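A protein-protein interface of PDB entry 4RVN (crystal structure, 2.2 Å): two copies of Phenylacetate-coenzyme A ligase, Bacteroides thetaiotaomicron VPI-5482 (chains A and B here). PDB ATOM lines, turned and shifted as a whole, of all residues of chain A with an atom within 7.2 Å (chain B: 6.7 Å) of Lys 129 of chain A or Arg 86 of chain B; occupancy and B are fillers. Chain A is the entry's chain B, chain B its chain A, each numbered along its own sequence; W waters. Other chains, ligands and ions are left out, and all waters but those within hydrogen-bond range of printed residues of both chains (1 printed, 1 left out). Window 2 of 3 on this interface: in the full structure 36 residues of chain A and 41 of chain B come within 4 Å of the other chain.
Of the 14 printed residues of chain A, 5 touch a printed residue of chain B.
Hydrophobic or aromatic side chains of chain A within 4 Å of the printed part of chain B: Leu 158.
Of the 8 printed residues of chain B, 5 touch a printed residue of chain A.
Printed residues of chain B that touch a printed residue of chain A: Met 84, Lys 85, Arg 86, Gly 88 and Val 89.
Among the printed residues, no Asp or Glu carboxylate lies within 4 Å of a Lys or Arg side-chain nitrogen of the other chain.
No position is printed for both chains.
Of the 10 pairs that touch across the chains among the printed residues, none has its exchanged pair printed and touching as well.
O of Lys 129 of chain A lies close to O of Lys 85 of chain B, 3.2 Å away.
The backbone carbonyl oxygen (O) of Gly 88 of chain B lies close to the backbone carbonyl oxygen (O) of Gly 156 of chain A (3.4 Å).
The backbone carbonyl oxygen (O) of Cys 157 of chain A sits close to the backbone carbonyl oxygen (O) of Val 89 of chain B, 3.2 Å away.
Printed residues of chain B within 4 Å of Lys 129 of chain A: Lys 85 and Arg 86.
Printed residues of chain A within 4 Å of Arg 86 of chain B: Lys 129 (3.2 Å).
Printed residues of chain A within 4 Å of Met 84 of chain B: Leu 158 (3.8 Å).
Of the printed residues of chain A, Lys 85 of chain B touches Lys 129 (3.2 Å) and Thr 130 (3.4 Å).
Printed residues of chain B within 4 Å of Thr 130 of chain A: Lys 85.
Of the printed residues of chain B, Cys 157 of chain A touches Gly 88 and Val 89.
Printed residues of chain B within 4 Å of Leu 158 of chain A: Met 84, Gly 88 and Val 89.
Asp 83 of chain B touches none of the printed residues of chain A.
The nearest printed residue of chain B that does not touch Lys 129 of chain A is Gly 88 of chain B (4.9 Å).
Water W1 bridges O of Gly 156 of chain A (2.5 Å) and O of Arg 86 of chain B (2.6 Å).
The side-chain carboxylate (OD2) of Asp 83 of chain B lies within salt-bridge range of the guanidinium group (NE) of Arg 86 of chain B (3.6 Å).
The backbone carbonyl oxygen of Asp 83 of chain B lies within hydrogen-bond range of the backbone NH of Gly 88 of chain B.
The backbone NH of Met 84 of chain B lies close to the side-chain sulfur of Met 295 of chain B (3.8 Å).
The guanidinium group (NH2) of Arg 86 of chain B lies within salt-bridge range of the side-chain carboxylate (OD2) of Asp 87 of chain B, 3.0 Å away.
The backbone carbonyl oxygen (O) of Arg 128 of chain A lies within hydrogen-bond range of the side-chain sulfur (SG) of Cys 157 of chain A (3.3 Å).
The backbone carbonyl oxygen (O) of Asp 131 of chain A is in hydrogen-bond range of the backbone NH (N) of Leu 158 of chain A (3.0 Å).
Arg 86 of chain B touches Lys 129 of chain A.
Thr 130 of chain A touches Lys 85 of chain B (CA to O, 3.4 Å).
Gly 156 of chain A touches Val 89 of chain B (O to CG1, 3.98 Å).
O of Cys 157 of chain A touches O of Gly 88 of chain B (3.6 Å).
Leu 158 of chain A touches Met 84 of chain B.
Gly 88 of chain B touches Leu 158 of chain A.
Leu 158 of chain A touches Val 89 of chain B.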
ATOM      1  N   TYR A 123     -32.781  -0.844 -22.456  1.00  0.00           N
ATOM      2  CA  TYR A 123     -32.343  -1.678 -23.578  1.00  0.00           C
ATOM      3  C   TYR A 123     -33.370  -2.787 -23.863  1.00  0.00           C
ATOM      4  O   TYR A 123     -33.626  -3.097 -25.026  1.00  0.00           O
ATOM      5  CB  TYR A 123     -30.959  -2.288 -23.285  1.00  0.00           C
ATOM      6  CG  TYR A 123     -30.307  -2.950 -24.480  1.00  0.00           C
ATOM      7  CD1 TYR A 123     -30.550  -4.287 -24.781  1.00  0.00           C
ATOM      8  CD2 TYR A 123     -29.418  -2.251 -25.289  1.00  0.00           C
ATOM      9  CE1 TYR A 123     -29.962  -4.899 -25.886  1.00  0.00           C
ATOM     10  CE2 TYR A 123     -28.806  -2.859 -26.386  1.00  0.00           C
ATOM     11  CZ  TYR A 123     -29.087  -4.182 -26.685  1.00  0.00           C
ATOM     12  OH  TYR A 123     -28.493  -4.789 -27.767  1.00  0.00           O
ATOM     13  N   GLY A 126     -36.284  -1.890 -26.050  1.00  0.00           N
ATOM     14  CA  GLY A 126     -35.838  -1.491 -27.386  1.00  0.00           C
ATOM     15  C   GLY A 126     -35.120  -0.162 -27.545  1.00  0.00           C
ATOM     16  O   GLY A 126     -34.812   0.226 -28.678  1.00  0.00           O
ATOM     17  N   ILE A 127     -34.844   0.550 -26.433  1.00  0.00           N
ATOM     18  CA  ILE A 127     -34.139   1.836 -26.486  1.00  0.00           C
ATOM     19  C   ILE A 127     -32.640   1.543 -26.692  1.00  0.00           C
ATOM     20  O   ILE A 127     -32.096   0.615 -26.088  1.00  0.00           O
ATOM     21  CB  ILE A 127     -34.424   2.709 -25.226  1.00  0.00           C
ATOM     22  CG1 ILE A 127     -35.949   2.972 -25.076  1.00  0.00           C
ATOM     23  CG2 ILE A 127     -33.636   4.033 -25.262  1.00  0.00           C
ATOM     24  CD1 ILE A 127     -36.420   3.597 -23.738  1.00  0.00           C
ATOM     25  N   ARG A 128     -32.002   2.305 -27.590  1.00  0.00           N
ATOM     26  CA  ARG A 128     -30.589   2.161 -27.941  1.00  0.00           C
ATOM     27  C   ARG A 128     -29.853   3.494 -27.757  1.00  0.00           C
ATOM     28  O   ARG A 128     -30.484   4.507 -27.453  1.00  0.00           O
ATOM     29  CB  ARG A 128     -30.440   1.653 -29.399  1.00  0.00           C
ATOM     30  CG  ARG A 128     -31.066   0.275 -29.680  1.00  0.00           C
ATOM     31  CD  ARG A 128     -30.336  -0.869 -28.993  1.00  0.00           C
ATOM     32  NE  ARG A 128     -30.973  -2.168 -29.232  1.00  0.00           N
ATOM     33  CZ  ARG A 128     -31.865  -2.740 -28.427  1.00  0.00           C
ATOM     34  NH1 ARG A 128     -32.243  -2.137 -27.304  1.00  0.00           N
ATOM     35  NH2 ARG A 128     -32.381  -3.922 -28.734  1.00  0.00           N
ATOM     36  N   LYS A 129     -28.519   3.493 -27.944  1.00  0.00           N
ATOM     37  CA  LYS A 129     -27.671   4.682 -27.811  1.00  0.00           C
ATOM     38  C   LYS A 129     -28.053   5.745 -28.867  1.00  0.00           C
ATOM     39  O   LYS A 129     -27.821   6.929 -28.636  1.00  0.00           O
ATOM     40  CB  LYS A 129     -26.175   4.311 -27.920  1.00  0.00           C
ATOM     41  CG  LYS A 129     -25.750   3.665 -29.247  1.00  0.00           C
ATOM     42  CD  LYS A 129     -24.364   3.007 -29.199  1.00  0.00           C
ATOM     43  CE  LYS A 129     -23.204   3.957 -29.016  1.00  0.00           C
ATOM     44  NZ  LYS A 129     -21.901   3.244 -29.006  1.00  0.00           N
ATOM     45  N   THR A 130     -28.673   5.317 -29.993  1.00  0.00           N
ATOM     46  CA  THR A 130     -29.121   6.177 -31.095  1.00  0.00           C
ATOM     47  C   THR A 130     -30.396   6.967 -30.727  1.00  0.00           C
ATOM     48  O   THR A 130     -30.736   7.928 -31.424  1.00  0.00           O
ATOM     49  CB  THR A 130     -29.372   5.343 -32.355  1.00  0.00           C
ATOM     50  OG1 THR A 130     -30.330   4.318 -32.067  1.00  0.00           O
ATOM     51  CG2 THR A 130     -28.092   4.735 -32.922  1.00  0.00           C
ATOM     52  N   ASP A 131     -31.097   6.568 -29.645  1.00  0.00           N
ATOM     53  CA  ASP A 131     -32.309   7.249 -29.199  1.00  0.00           C
ATOM     54  C   ASP A 131     -31.994   8.566 -28.483  1.00  0.00           C
ATOM     55  O   ASP A 131     -30.915   8.732 -27.910  1.00  0.00           O
ATOM     56  CB  ASP A 131     -33.137   6.348 -28.261  1.00  0.00           C
ATOM     57  CG  ASP A 131     -33.905   5.259 -28.988  1.00  0.00           C
ATOM     58  OD1 ASP A 131     -34.994   5.561 -29.526  1.00  0.00           O
ATOM     59  OD2 ASP A 131     -33.430   4.104 -29.002  1.00  0.00           O
ATOM     60  N   VAL A 132     -32.966   9.496 -28.527  1.00  0.00           N
ATOM     61  CA  VAL A 132     -32.933  10.782 -27.833  1.00  0.00           C
ATOM     62  C   VAL A 132     -33.884  10.615 -26.642  1.00  0.00           C
ATOM     63  O   VAL A 132     -35.098  10.510 -26.839  1.00  0.00           O
ATOM     64  CB  VAL A 132     -33.265  11.988 -28.760  1.00  0.00           C
ATOM     65  CG1 VAL A 132     -33.216  13.308 -27.993  1.00  0.00           C
ATOM     66  CG2 VAL A 132     -32.322  12.038 -29.963  1.00  0.00           C
ATOM     67  N   ALA A 152     -29.571   6.251 -18.719  1.00  0.00           N
ATOM     68  CA  ALA A 152     -29.647   6.583 -20.144  1.00  0.00           C
ATOM     69  C   ALA A 152     -28.273   6.985 -20.692  1.00  0.00           C
ATOM     70  O   ALA A 152     -27.968   6.628 -21.828  1.00  0.00           O
ATOM     71  CB  ALA A 152     -30.652   7.689 -20.387  1.00  0.00           C
ATOM     72  N   ARG A 154     -25.388   5.836 -19.456  1.00  0.00           N
ATOM     73  CA  ARG A 154     -24.693   4.539 -19.439  1.00  0.00           C
ATOM     74  C   ARG A 154     -25.001   3.771 -20.738  1.00  0.00           C
ATOM     75  O   ARG A 154     -24.093   3.188 -21.334  1.00  0.00           O
ATOM     76  CB  ARG A 154     -25.101   3.716 -18.192  1.00  0.00           C
ATOM     77  CG  ARG A 154     -24.529   2.293 -18.133  1.00  0.00           C
ATOM     78  CD  ARG A 154     -23.047   2.233 -17.803  1.00  0.00           C
ATOM     79  NE  ARG A 154     -22.814   2.290 -16.359  1.00  0.00           N
ATOM     80  CZ  ARG A 154     -22.783   1.220 -15.566  1.00  0.00           C
ATOM     81  NH1 ARG A 154     -22.976   0.006 -16.070  1.00  0.00           N
ATOM     82  NH2 ARG A 154     -22.568   1.358 -14.265  1.00  0.00           N
ATOM     83  N   LEU A 155     -26.277   3.806 -21.184  1.00  0.00           N
ATOM     84  CA  LEU A 155     -26.727   3.177 -22.427  1.00  0.00           C
ATOM     85  C   LEU A 155     -26.131   3.940 -23.640  1.00  0.00           C
ATOM     86  O   LEU A 155     -25.792   3.319 -24.646  1.00  0.00           O
ATOM     87  CB  LEU A 155     -28.274   3.133 -22.476  1.00  0.00           C
ATOM     88  CG  LEU A 155     -28.975   2.552 -23.724  1.00  0.00           C
ATOM     89  CD1 LEU A 155     -28.457   1.169 -24.091  1.00  0.00           C
ATOM     90  CD2 LEU A 155     -30.476   2.479 -23.511  1.00  0.00           C
ATOM     91  N   GLY A 156     -25.976   5.257 -23.505  1.00  0.00           N
ATOM     92  CA  GLY A 156     -25.392   6.100 -24.544  1.00  0.00           C
ATOM     93  C   GLY A 156     -26.366   6.996 -25.278  1.00  0.00           C
ATOM     94  O   GLY A 156     -25.992   7.616 -26.274  1.00  0.00           O
ATOM     95  N   CYS A 157     -27.620   7.069 -24.795  1.00  0.00           N
ATOM     96  CA  CYS A 157     -28.681   7.918 -25.350  1.00  0.00           C
ATOM     97  C   CYS A 157     -28.279   9.379 -25.325  1.00  0.00           C
ATOM     98  O   CYS A 157     -27.595   9.806 -24.390  1.00  0.00           O
ATOM     99  CB  CYS A 157     -29.980   7.737 -24.565  1.00  0.00           C
ATOM    100  SG  CYS A 157     -30.617   6.046 -24.512  1.00  0.00           S
ATOM    101  N   LEU A 158     -28.796  10.164 -26.282  1.00  0.00           N
ATOM    102  CA  LEU A 158     -28.668  11.613 -26.245  1.00  0.00           C
ATOM    103  C   LEU A 158     -29.717  12.078 -25.245  1.00  0.00           C
ATOM    104  O   LEU A 158     -30.905  12.052 -25.564  1.00  0.00           O
ATOM    105  CB  LEU A 158     -28.817  12.236 -27.652  1.00  0.00           C
ATOM    106  CG  LEU A 158     -28.774  13.766 -27.738  1.00  0.00           C
ATOM    107  CD1 LEU A 158     -27.400  14.312 -27.357  1.00  0.00           C
ATOM    108  CD2 LEU A 158     -29.155  14.230 -29.131  1.00  0.00           C
ATOM    109  N   ASP B  83     -20.204  12.891 -33.892  1.00  0.00           N
ATOM    110  CA  ASP B  83     -21.291  11.982 -34.261  1.00  0.00           C
ATOM    111  C   ASP B  83     -22.259  11.933 -33.080  1.00  0.00           C
ATOM    112  O   ASP B  83     -22.055  11.185 -32.117  1.00  0.00           O
ATOM    113  CB  ASP B  83     -20.748  10.592 -34.653  1.00  0.00           C
ATOM    114  CG  ASP B  83     -21.765   9.595 -35.202  1.00  0.00           C
ATOM    115  OD1 ASP B  83     -22.988   9.876 -35.128  1.00  0.00           O
ATOM    116  OD2 ASP B  83     -21.340   8.533 -35.692  1.00  0.00           O
ATOM    117  N   MET B  84     -23.286  12.782 -33.141  1.00  0.00           N
ATOM    118  CA  MET B  84     -24.265  12.975 -32.086  1.00  0.00           C
ATOM    119  C   MET B  84     -25.119  11.715 -31.856  1.00  0.00           C
ATOM    120  O   MET B  84     -25.356  11.356 -30.707  1.00  0.00           O
ATOM    121  CB  MET B  84     -25.155  14.170 -32.440  1.00  0.00           C
ATOM    122  CG  MET B  84     -26.075  14.602 -31.310  1.00  0.00           C
ATOM    123  SD  MET B  84     -27.017  16.240 -31.696  1.00  0.00           S
ATOM    124  CE  MET B  84     -28.000  15.677 -33.304  1.00  0.00           C
ATOM    125  N   LYS B  85     -25.551  11.041 -32.922  1.00  0.00           N
ATOM    126  CA  LYS B  85     -26.395   9.846 -32.816  1.00  0.00           C
ATOM    127  C   LYS B  85     -25.672   8.708 -32.078  1.00  0.00           C
ATOM    128  O   LYS B  85     -26.293   8.042 -31.253  1.00  0.00           O
ATOM    129  CB  LYS B  85     -26.826   9.373 -34.216  1.00  0.00           C
ATOM    130  CG  LYS B  85     -28.056   8.469 -34.206  1.00  0.00           C
ATOM    131  CD  LYS B  85     -28.960   8.758 -35.402  1.00  0.00           C
ATOM    132  CE  LYS B  85     -30.328   8.125 -35.302  1.00  0.00           C
ATOM    133  NZ  LYS B  85     -31.260   8.676 -36.324  1.00  0.00           N
ATOM    134  N   ARG B  86     -24.361   8.529 -32.345  1.00  0.00           N
ATOM    135  CA  ARG B  86     -23.538   7.477 -31.752  1.00  0.00           C
ATOM    136  C   ARG B  86     -22.877   7.908 -30.425  1.00  0.00           C
ATOM    137  O   ARG B  86     -22.883   7.131 -29.471  1.00  0.00           O
ATOM    138  CB  ARG B  86     -22.441   7.074 -32.754  1.00  0.00           C
ATOM    139  CG  ARG B  86     -21.570   5.882 -32.349  1.00  0.00           C
ATOM    140  CD  ARG B  86     -20.396   5.707 -33.299  1.00  0.00           C
ATOM    141  NE  ARG B  86     -19.447   6.821 -33.204  1.00  0.00           N
ATOM    142  CZ  ARG B  86     -18.388   6.984 -33.990  1.00  0.00           C
ATOM    143  NH1 ARG B  86     -18.131   6.113 -34.959  1.00  0.00           N
ATOM    144  NH2 ARG B  86     -17.586   8.026 -33.824  1.00  0.00           N
ATOM    145  N   ASP B  87     -22.264   9.112 -30.371  1.00  0.00           N
ATOM    146  CA  ASP B  87     -21.505   9.528 -29.191  1.00  0.00           C
ATOM    147  C   ASP B  87     -22.140  10.665 -28.348  1.00  0.00           C
ATOM    148  O   ASP B  87     -21.649  10.903 -27.248  1.00  0.00           O
ATOM    149  CB  ASP B  87     -20.109  10.002 -29.653  1.00  0.00           C
ATOM    150  CG  ASP B  87     -19.313   8.951 -30.427  1.00  0.00           C
ATOM    151  OD1 ASP B  87     -19.383   7.758 -30.061  1.00  0.00           O
ATOM    152  OD2 ASP B  87     -18.589   9.329 -31.368  1.00  0.00           O
ATOM    153  N   GLY B  88     -23.194  11.324 -28.826  1.00  0.00           N
ATOM    154  CA  GLY B  88     -23.858  12.388 -28.068  1.00  0.00           C
ATOM    155  C   GLY B  88     -24.621  11.815 -26.895  1.00  0.00           C
ATOM    156  O   GLY B  88     -25.440  10.908 -27.087  1.00  0.00           O
ATOM    157  N   VAL B  89     -24.329  12.287 -25.662  1.00  0.00           N
ATOM    158  CA  VAL B  89     -24.974  11.717 -24.469  1.00  0.00           C
ATOM    159  C   VAL B  89     -25.787  12.788 -23.679  1.00  0.00           C
ATOM    160  O   VAL B  89     -26.582  12.395 -22.822  1.00  0.00           O
ATOM    161  CB  VAL B  89     -23.979  10.995 -23.513  1.00  0.00           C
ATOM    162  CG1 VAL B  89     -23.371   9.761 -24.176  1.00  0.00           C
ATOM    163  CG2 VAL B  89     -22.891  11.931 -23.003  1.00  0.00           C
ATOM    164  N   MET B 295     -17.563  17.030 -28.978  1.00  0.00           N
ATOM    165  CA  MET B 295     -18.872  16.955 -29.651  1.00  0.00           C
ATOM    166  C   MET B 295     -19.233  18.307 -30.282  1.00  0.00           C
ATOM    167  O   MET B 295     -19.614  18.359 -31.455  1.00  0.00           O
ATOM    168  CB  MET B 295     -19.967  16.514 -28.669  1.00  0.00           C
ATOM    169  CG  MET B 295     -21.369  16.397 -29.299  1.00  0.00           C
ATOM    170  SD  MET B 295     -21.512  15.233 -30.874  1.00  0.00           S
ATOM    171  CE  MET B 295     -20.822  13.622 -30.091  1.00  0.00           C
HETATM  172  O   HOH W   1     -23.612   7.774 -27.095  1.00  0.00           O
